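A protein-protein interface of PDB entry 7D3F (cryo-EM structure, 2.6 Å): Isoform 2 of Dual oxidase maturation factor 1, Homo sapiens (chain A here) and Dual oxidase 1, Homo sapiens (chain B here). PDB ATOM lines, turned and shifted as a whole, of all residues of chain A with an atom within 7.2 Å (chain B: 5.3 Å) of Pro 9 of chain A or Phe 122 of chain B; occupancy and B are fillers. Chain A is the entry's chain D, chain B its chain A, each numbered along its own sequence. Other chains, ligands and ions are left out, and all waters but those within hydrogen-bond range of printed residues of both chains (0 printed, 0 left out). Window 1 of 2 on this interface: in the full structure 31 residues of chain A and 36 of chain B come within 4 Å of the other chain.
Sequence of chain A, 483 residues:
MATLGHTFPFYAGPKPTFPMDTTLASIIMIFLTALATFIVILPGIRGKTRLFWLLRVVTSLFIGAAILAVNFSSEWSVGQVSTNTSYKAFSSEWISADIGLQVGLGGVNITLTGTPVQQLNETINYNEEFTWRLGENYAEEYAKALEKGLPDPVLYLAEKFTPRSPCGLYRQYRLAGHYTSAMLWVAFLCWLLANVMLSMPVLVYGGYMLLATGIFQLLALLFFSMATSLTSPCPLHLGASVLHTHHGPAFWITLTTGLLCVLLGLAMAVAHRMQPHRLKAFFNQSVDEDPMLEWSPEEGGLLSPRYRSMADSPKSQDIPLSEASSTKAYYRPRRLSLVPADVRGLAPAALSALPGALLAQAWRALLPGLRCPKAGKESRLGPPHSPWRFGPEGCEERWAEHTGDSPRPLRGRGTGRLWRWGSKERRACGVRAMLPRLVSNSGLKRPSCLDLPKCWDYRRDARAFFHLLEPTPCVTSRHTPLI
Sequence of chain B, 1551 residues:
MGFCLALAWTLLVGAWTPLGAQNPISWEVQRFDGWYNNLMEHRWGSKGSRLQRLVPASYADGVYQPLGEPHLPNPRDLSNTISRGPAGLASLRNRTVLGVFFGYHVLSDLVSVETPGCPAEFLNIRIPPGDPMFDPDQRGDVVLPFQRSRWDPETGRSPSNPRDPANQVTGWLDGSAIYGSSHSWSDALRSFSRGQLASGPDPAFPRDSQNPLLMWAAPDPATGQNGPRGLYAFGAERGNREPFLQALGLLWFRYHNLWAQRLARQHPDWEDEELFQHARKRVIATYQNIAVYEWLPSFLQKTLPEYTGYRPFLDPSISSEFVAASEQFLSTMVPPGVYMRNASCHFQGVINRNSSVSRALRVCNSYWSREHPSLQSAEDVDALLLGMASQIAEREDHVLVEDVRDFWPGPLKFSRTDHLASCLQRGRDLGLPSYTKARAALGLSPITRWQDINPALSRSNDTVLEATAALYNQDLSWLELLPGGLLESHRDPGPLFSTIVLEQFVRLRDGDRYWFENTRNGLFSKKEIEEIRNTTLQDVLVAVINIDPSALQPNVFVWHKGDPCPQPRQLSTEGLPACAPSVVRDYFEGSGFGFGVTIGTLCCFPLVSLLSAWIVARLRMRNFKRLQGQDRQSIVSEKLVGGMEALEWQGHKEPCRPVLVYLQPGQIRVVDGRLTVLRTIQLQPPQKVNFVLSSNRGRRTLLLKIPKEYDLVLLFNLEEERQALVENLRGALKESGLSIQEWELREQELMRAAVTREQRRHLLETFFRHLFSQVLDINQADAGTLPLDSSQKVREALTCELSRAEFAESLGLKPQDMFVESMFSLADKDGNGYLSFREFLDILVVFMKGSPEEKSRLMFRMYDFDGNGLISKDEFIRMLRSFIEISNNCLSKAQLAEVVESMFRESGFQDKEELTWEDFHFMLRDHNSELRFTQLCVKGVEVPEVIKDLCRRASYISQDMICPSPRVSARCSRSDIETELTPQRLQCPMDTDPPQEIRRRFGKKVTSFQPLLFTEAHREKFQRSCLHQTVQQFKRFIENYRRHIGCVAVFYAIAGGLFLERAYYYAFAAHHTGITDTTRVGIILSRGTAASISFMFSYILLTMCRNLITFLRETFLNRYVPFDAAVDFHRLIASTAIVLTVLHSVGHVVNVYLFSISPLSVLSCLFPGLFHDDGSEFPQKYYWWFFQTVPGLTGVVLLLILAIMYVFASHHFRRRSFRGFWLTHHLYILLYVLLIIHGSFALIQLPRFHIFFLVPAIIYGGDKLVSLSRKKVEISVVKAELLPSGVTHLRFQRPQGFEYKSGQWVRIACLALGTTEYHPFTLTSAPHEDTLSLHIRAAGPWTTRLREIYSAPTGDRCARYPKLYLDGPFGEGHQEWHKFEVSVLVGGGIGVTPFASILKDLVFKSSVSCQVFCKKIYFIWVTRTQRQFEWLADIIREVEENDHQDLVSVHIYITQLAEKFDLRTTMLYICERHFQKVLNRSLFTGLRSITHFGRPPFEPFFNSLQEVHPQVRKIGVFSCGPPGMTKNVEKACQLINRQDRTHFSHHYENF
ND2 of Asn 124 of chain B sits at hydrogen-bond distance from O of Phe 8 of chain A. The backbone carbonyl oxygen of Asp 1077 of chain B sits at hydrogen-bond distance from the backbone NH of Phe 10 of chain A, 3.1 Å away. O of Asp 1077 of chain B is in hydrogen-bond range of N of Tyr 11 of chain A, at 3.0 Å.
The side-chain amide oxygen (OD1) of Asn 124 of chain B lies within hydrogen-bond range of the backbone NH (N) of Phe 146 of chain B (3.5 Å).
Among the printed residues, pairs that only touch across the chains: Phe 8 of chain A with Pro 1159 of chain B (3.5 Å), Pro 9 of chain A with Asp 1077 of chain B (3.5 Å), Phe 8 of chain A with Phe 122 of chain B (3.5 Å), Phe 8 of chain A with Leu 412 of chain B (3.8 Å) and Pro 9 of chain A with Phe 122 of chain B (3.97 Å).
Phe 122 of chain B touches two residues of chain A. Of the printed residues of chain A, Leu 412 of chain B touches Phe 8 (3.8 Å). Printed residues of chain B within 4 Å of Phe 10 of chain A: Asp 1077. Printed residues of chain A within 4 Å of Asp 1077 of chain B: Pro 9, Phe 10 and Tyr 11. Of the printed residues of chain A, Pro 1159 of chain B touches Phe 8. Of the printed residues of chain B, Tyr 11 of chain A touches Asp 1077. The nearest residue of chain A that does not touch Phe 122 of chain B is Phe 10 of chain A (6.5 Å). The nearest printed residue of chain A that does not touch Asn 124 of chain B is Thr 7 of chain A (4.4 Å).
Along chain B the printed residues that touch a printed residue of chain A span positions 122 to 1159. Hydrophobic or aromatic side chains of chain A within 4 Å of the printed part of chain B: Phe 8, Pro 9, Phe 10 and Tyr 11. Among the printed residues, 8 pairs touch across the chains.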
ATOM      1  N   LEU A   4     -29.510  17.063 -22.719  1.00  0.00           N
ATOM      2  CA  LEU A   4     -29.277  17.997 -21.625  1.00  0.00           C
ATOM      3  C   LEU A   4     -29.322  19.428 -22.134  1.00  0.00           C
ATOM      4  O   LEU A   4     -28.812  19.751 -23.214  1.00  0.00           O
ATOM      5  CB  LEU A   4     -27.939  17.717 -20.939  1.00  0.00           C
ATOM      6  N   THR A   7     -27.798  25.063 -20.650  1.00  0.00           N
ATOM      7  CA  THR A   7     -26.530  25.702 -20.955  1.00  0.00           C
ATOM      8  C   THR A   7     -26.380  25.792 -22.467  1.00  0.00           C
ATOM      9  O   THR A   7     -26.991  25.028 -23.221  1.00  0.00           O
ATOM     10  CB  THR A   7     -25.342  24.943 -20.346  1.00  0.00           C
ATOM     11  OG1 THR A   7     -24.139  25.688 -20.559  1.00  0.00           O
ATOM     12  CG2 THR A   7     -25.198  23.568 -20.982  1.00  0.00           C
ATOM     13  N   PHE A   8     -25.559  26.742 -22.911  1.00  0.00           N
ATOM     14  CA  PHE A   8     -25.389  26.963 -24.336  1.00  0.00           C
ATOM     15  C   PHE A   8     -23.914  27.073 -24.694  1.00  0.00           C
ATOM     16  O   PHE A   8     -23.144  27.720 -23.972  1.00  0.00           O
ATOM     17  CB  PHE A   8     -26.124  28.232 -24.785  1.00  0.00           C
ATOM     18  CG  PHE A   8     -27.550  28.298 -24.325  1.00  0.00           C
ATOM     19  CD1 PHE A   8     -28.471  27.352 -24.744  1.00  0.00           C
ATOM     20  CD2 PHE A   8     -27.971  29.306 -23.477  1.00  0.00           C
ATOM     21  CE1 PHE A   8     -29.784  27.408 -24.320  1.00  0.00           C
ATOM     22  CE2 PHE A   8     -29.282  29.370 -23.053  1.00  0.00           C
ATOM     23  CZ  PHE A   8     -30.191  28.419 -23.474  1.00  0.00           C
ATOM     24  N   PRO A   9     -23.486  26.451 -25.804  1.00  0.00           N
ATOM     25  CA  PRO A   9     -24.343  25.608 -26.646  1.00  0.00           C
ATOM     26  C   PRO A   9     -24.515  24.202 -26.075  1.00  0.00           C
ATOM     27  O   PRO A   9     -23.778  23.818 -25.166  1.00  0.00           O
ATOM     28  CB  PRO A   9     -23.592  25.570 -27.976  1.00  0.00           C
ATOM     29  CG  PRO A   9     -22.164  25.701 -27.584  1.00  0.00           C
ATOM     30  CD  PRO A   9     -22.138  26.608 -26.379  1.00  0.00           C
ATOM     31  N   PHE A  10     -25.486  23.452 -26.601  1.00  0.00           N
ATOM     32  CA  PHE A  10     -25.696  22.085 -26.133  1.00  0.00           C
ATOM     33  C   PHE A  10     -24.483  21.213 -26.427  1.00  0.00           C
ATOM     34  O   PHE A  10     -24.100  20.369 -25.608  1.00  0.00           O
ATOM     35  CB  PHE A  10     -26.953  21.496 -26.774  1.00  0.00           C
ATOM     36  CG  PHE A  10     -28.217  22.228 -26.416  1.00  0.00           C
ATOM     37  CD1 PHE A  10     -28.306  22.952 -25.239  1.00  0.00           C
ATOM     38  CD2 PHE A  10     -29.316  22.191 -27.258  1.00  0.00           C
ATOM     39  CE1 PHE A  10     -29.465  23.626 -24.909  1.00  0.00           C
ATOM     40  CE2 PHE A  10     -30.478  22.863 -26.933  1.00  0.00           C
ATOM     41  CZ  PHE A  10     -30.552  23.582 -25.757  1.00  0.00           C
ATOM     42  N   TYR A  11     -23.866  21.403 -27.589  1.00  0.00           N
ATOM     43  CA  TYR A  11     -22.648  20.696 -27.977  1.00  0.00           C
ATOM     44  C   TYR A  11     -21.556  21.743 -28.175  1.00  0.00           C
ATOM     45  O   TYR A  11     -21.456  22.351 -29.245  1.00  0.00           O
ATOM     46  CB  TYR A  11     -22.872  19.868 -29.240  1.00  0.00           C
ATOM     47  CG  TYR A  11     -23.976  18.842 -29.110  1.00  0.00           C
ATOM     48  CD1 TYR A  11     -25.297  19.178 -29.379  1.00  0.00           C
ATOM     49  CD2 TYR A  11     -23.698  17.539 -28.721  1.00  0.00           C
ATOM     50  CE1 TYR A  11     -26.309  18.244 -29.261  1.00  0.00           C
ATOM     51  CE2 TYR A  11     -24.705  16.598 -28.601  1.00  0.00           C
ATOM     52  CZ  TYR A  11     -26.008  16.957 -28.874  1.00  0.00           C
ATOM     53  OH  TYR A  11     -27.015  16.027 -28.756  1.00  0.00           O
ATOM     54  N   ALA A  12     -20.741  21.951 -27.143  1.00  0.00           N
ATOM     55  CA  ALA A  12     -19.715  22.985 -27.156  1.00  0.00           C
ATOM     56  C   ALA A  12     -18.363  22.483 -27.644  1.00  0.00           C
ATOM     57  O   ALA A  12     -17.407  23.265 -27.678  1.00  0.00           O
ATOM     58  CB  ALA A  12     -19.562  23.593 -25.758  1.00  0.00           C
ATOM     59  N   GLY A  13     -18.257  21.212 -28.018  1.00  0.00           N
ATOM     60  CA  GLY A  13     -17.014  20.667 -28.510  1.00  0.00           C
ATOM     61  C   GLY A  13     -16.646  21.221 -29.871  1.00  0.00           C
ATOM     62  O   GLY A  13     -17.502  21.698 -30.624  1.00  0.00           O
ATOM     63  N   ALA B 120     -25.216  31.030 -34.045  1.00  0.00           N
ATOM     64  CA  ALA B 120     -25.219  31.361 -32.627  1.00  0.00           C
ATOM     65  C   ALA B 120     -23.920  30.944 -31.954  1.00  0.00           C
ATOM     66  O   ALA B 120     -23.633  29.751 -31.822  1.00  0.00           O
ATOM     67  CB  ALA B 120     -26.409  30.698 -31.935  1.00  0.00           C
ATOM     68  N   GLU B 121     -23.133  31.926 -31.526  1.00  0.00           N
ATOM     69  CA  GLU B 121     -21.889  31.694 -30.808  1.00  0.00           C
ATOM     70  C   GLU B 121     -22.034  32.227 -29.391  1.00  0.00           C
ATOM     71  O   GLU B 121     -22.500  33.354 -29.191  1.00  0.00           O
ATOM     72  CB  GLU B 121     -20.711  32.372 -31.509  1.00  0.00           C
ATOM     73  CG  GLU B 121     -20.657  32.138 -33.008  1.00  0.00           C
ATOM     74  CD  GLU B 121     -19.529  32.900 -33.674  1.00  0.00           C
ATOM     75  OE1 GLU B 121     -18.355  32.644 -33.333  1.00  0.00           O
ATOM     76  OE2 GLU B 121     -19.820  33.761 -34.532  1.00  0.00           O
ATOM     77  N   PHE B 122     -21.629  31.423 -28.415  1.00  0.00           N
ATOM     78  CA  PHE B 122     -21.767  31.770 -27.009  1.00  0.00           C
ATOM     79  C   PHE B 122     -20.394  31.945 -26.379  1.00  0.00           C
ATOM     80  O   PHE B 122     -19.553  31.042 -26.449  1.00  0.00           O
ATOM     81  CB  PHE B 122     -22.563  30.701 -26.256  1.00  0.00           C
ATOM     82  CG  PHE B 122     -24.014  30.648 -26.641  1.00  0.00           C
ATOM     83  CD1 PHE B 122     -24.944  31.435 -25.984  1.00  0.00           C
ATOM     84  CD2 PHE B 122     -24.445  29.819 -27.664  1.00  0.00           C
ATOM     85  CE1 PHE B 122     -26.274  31.397 -26.338  1.00  0.00           C
ATOM     86  CE2 PHE B 122     -25.778  29.777 -28.021  1.00  0.00           C
ATOM     87  CZ  PHE B 122     -26.693  30.567 -27.356  1.00  0.00           C
ATOM     88  N   LEU B 123     -20.177  33.102 -25.761  1.00  0.00           N
ATOM     89  CA  LEU B 123     -18.971  33.387 -24.991  1.00  0.00           C
ATOM     90  C   LEU B 123     -19.416  33.545 -23.541  1.00  0.00           C
ATOM     91  O   LEU B 123     -19.630  34.652 -23.046  1.00  0.00           O
ATOM     92  CB  LEU B 123     -18.267  34.640 -25.520  1.00  0.00           C
ATOM     93  CG  LEU B 123     -16.809  34.842 -25.109  1.00  0.00           C
ATOM     94  CD1 LEU B 123     -15.941  33.726 -25.670  1.00  0.00           C
ATOM     95  CD2 LEU B 123     -16.308  36.200 -25.571  1.00  0.00           C
ATOM     96  N   ASN B 124     -19.542  32.412 -22.855  1.00  0.00           N
ATOM     97  CA  ASN B 124     -20.172  32.389 -21.543  1.00  0.00           C
ATOM     98  C   ASN B 124     -19.268  32.999 -20.481  1.00  0.00           C
ATOM     99  O   ASN B 124     -18.045  32.835 -20.509  1.00  0.00           O
ATOM    100  CB  ASN B 124     -20.536  30.954 -21.167  1.00  0.00           C
ATOM    101  CG  ASN B 124     -21.692  30.414 -21.985  1.00  0.00           C
ATOM    102  OD1 ASN B 124     -22.523  31.174 -22.481  1.00  0.00           O
ATOM    103  ND2 ASN B 124     -21.753  29.096 -22.125  1.00  0.00           N
ATOM    104  N   PRO B 145     -24.956  33.112 -19.480  1.00  0.00           N
ATOM    105  CA  PRO B 145     -24.829  32.995 -20.937  1.00  0.00           C
ATOM    106  C   PRO B 145     -24.667  34.356 -21.595  1.00  0.00           C
ATOM    107  O   PRO B 145     -25.317  35.335 -21.217  1.00  0.00           O
ATOM    108  CB  PRO B 145     -26.140  32.320 -21.356  1.00  0.00           C
ATOM    109  CG  PRO B 145     -27.099  32.668 -20.277  1.00  0.00           C
ATOM    110  CD  PRO B 145     -26.303  32.748 -19.007  1.00  0.00           C
ATOM    111  N   PHE B 146     -23.787  34.404 -22.591  1.00  0.00           N
ATOM    112  CA  PHE B 146     -23.504  35.617 -23.343  1.00  0.00           C
ATOM    113  C   PHE B 146     -23.290  35.232 -24.798  1.00  0.00           C
ATOM    114  O   PHE B 146     -22.560  34.278 -25.084  1.00  0.00           O
ATOM    115  CB  PHE B 146     -22.271  36.338 -22.780  1.00  0.00           C
ATOM    116  CG  PHE B 146     -21.828  37.524 -23.589  1.00  0.00           C
ATOM    117  CD1 PHE B 146     -22.341  38.784 -23.334  1.00  0.00           C
ATOM    118  CD2 PHE B 146     -20.883  37.381 -24.593  1.00  0.00           C
ATOM    119  CE1 PHE B 146     -21.929  39.878 -24.072  1.00  0.00           C
ATOM    120  CE2 PHE B 146     -20.468  38.469 -25.334  1.00  0.00           C
ATOM    121  CZ  PHE B 146     -20.991  39.719 -25.073  1.00  0.00           C
ATOM    122  N   GLN B 147     -23.920  35.965 -25.709  1.00  0.00           N
ATOM    123  CA  GLN B 147     -23.898  35.638 -27.127  1.00  0.00           C
ATOM    124  C   GLN B 147     -23.147  36.707 -27.907  1.00  0.00           C
ATOM    125  O   GLN B 147     -23.274  37.904 -27.625  1.00  0.00           O
ATOM    126  CB  GLN B 147     -25.320  35.489 -27.673  1.00  0.00           C
ATOM    127  CG  GLN B 147     -25.540  34.211 -28.464  1.00  0.00           C
ATOM    128  CD  GLN B 147     -26.957  34.077 -28.982  1.00  0.00           C
ATOM    129  OE1 GLN B 147     -27.917  34.459 -28.310  1.00  0.00           O
ATOM    130  NE2 GLN B 147     -27.097  33.543 -30.190  1.00  0.00           N
ATOM    131  N   ARG B 148     -22.364  36.267 -28.890  1.00  0.00           N
ATOM    132  CA  ARG B 148     -21.601  37.189 -29.718  1.00  0.00           C
ATOM    133  C   ARG B 148     -22.520  37.936 -30.679  1.00  0.00           C
ATOM    134  O   ARG B 148     -23.566  37.433 -31.094  1.00  0.00           O
ATOM    135  CB  ARG B 148     -20.520  36.436 -30.495  1.00  0.00           C
ATOM    136  CG  ARG B 148     -19.628  35.569 -29.618  1.00  0.00           C
ATOM    137  CD  ARG B 148     -18.440  35.020 -30.393  1.00  0.00           C
ATOM    138  NE  ARG B 148     -17.523  36.077 -30.807  1.00  0.00           N
ATOM    139  CZ  ARG B 148     -16.368  35.864 -31.429  1.00  0.00           C
ATOM    140  NH1 ARG B 148     -15.981  34.628 -31.710  1.00  0.00           N
ATOM    141  NH2 ARG B 148     -15.597  36.889 -31.769  1.00  0.00           N
ATOM    142  N   LEU B 412     -30.591  36.203 -21.607  1.00  0.00           N
ATOM    143  CA  LEU B 412     -30.689  34.765 -21.838  1.00  0.00           C
ATOM    144  C   LEU B 412     -30.714  34.013 -20.518  1.00  0.00           C
ATOM    145  O   LEU B 412     -29.778  34.127 -19.721  1.00  0.00           O
ATOM    146  CB  LEU B 412     -29.524  34.288 -22.705  1.00  0.00           C
ATOM    147  CG  LEU B 412     -29.829  33.051 -23.542  1.00  0.00           C
ATOM    148  CD1 LEU B 412     -31.251  33.142 -24.048  1.00  0.00           C
ATOM    149  CD2 LEU B 412     -28.863  32.956 -24.701  1.00  0.00           C
ATOM    150  N   ASP B1077     -24.475  22.724 -33.127  1.00  0.00           N
ATOM    151  CA  ASP B1077     -24.273  23.271 -31.792  1.00  0.00           C
ATOM    152  C   ASP B1077     -25.469  23.024 -30.884  1.00  0.00           C
ATOM    153  O   ASP B1077     -25.318  23.054 -29.658  1.00  0.00           O
ATOM    154  CB  ASP B1077     -23.978  24.768 -31.877  1.00  0.00           C
ATOM    155  CG  ASP B1077     -22.587  25.059 -32.407  1.00  0.00           C
ATOM    156  OD1 ASP B1077     -21.815  24.100 -32.621  1.00  0.00           O
ATOM    157  OD2 ASP B1077     -22.267  26.249 -32.605  1.00  0.00           O
ATOM    158  N   PRO B1159     -32.949  28.918 -27.172  1.00  0.00           N
ATOM    159  CA  PRO B1159     -33.497  30.278 -27.119  1.00  0.00           C
ATOM    160  C   PRO B1159     -33.971  30.744 -28.487  1.00  0.00           C
ATOM    161  O   PRO B1159     -33.715  30.122 -29.520  1.00  0.00           O
ATOM    162  CB  PRO B1159     -32.322  31.119 -26.619  1.00  0.00           C
ATOM    163  CG  PRO B1159     -31.117  30.347 -27.003  1.00  0.00           C
ATOM    164  CD  PRO B1159     -31.496  28.897 -26.937  1.00  0.00           C
ATOM    165  N   SER B1161     -33.058  33.381 -30.176  1.00  0.00           N
ATOM    166  CA  SER B1161     -31.971  33.793 -31.061  1.00  0.00           C
ATOM    167  C   SER B1161     -31.380  32.598 -31.801  1.00  0.00           C
ATOM    168  O   SER B1161     -31.112  32.670 -33.008  1.00  0.00           O
ATOM    169  CB  SER B1161     -30.890  34.515 -30.260  1.00  0.00           C
ATOM    170  OG  SER B1161     -30.369  33.680 -29.241  1.00  0.00           O
ATOM    171  N   VAL B1162     -31.173  31.487 -31.091  1.00  0.00           N
ATOM    172  CA  VAL B1162     -30.620  30.291 -31.716  1.00  0.00           C
ATOM    173  C   VAL B1162     -31.564  29.760 -32.787  1.00  0.00           C
ATOM    174  O   VAL B1162     -31.136  29.409 -33.892  1.00  0.00           O
ATOM    175  CB  VAL B1162     -30.314  29.224 -30.649  1.00  0.00           C
ATOM    176  CG1 VAL B1162     -30.064  27.885 -31.303  1.00  0.00           C
ATOM    177  CG2 VAL B1162     -29.114  29.640 -29.819  1.00  0.00           C
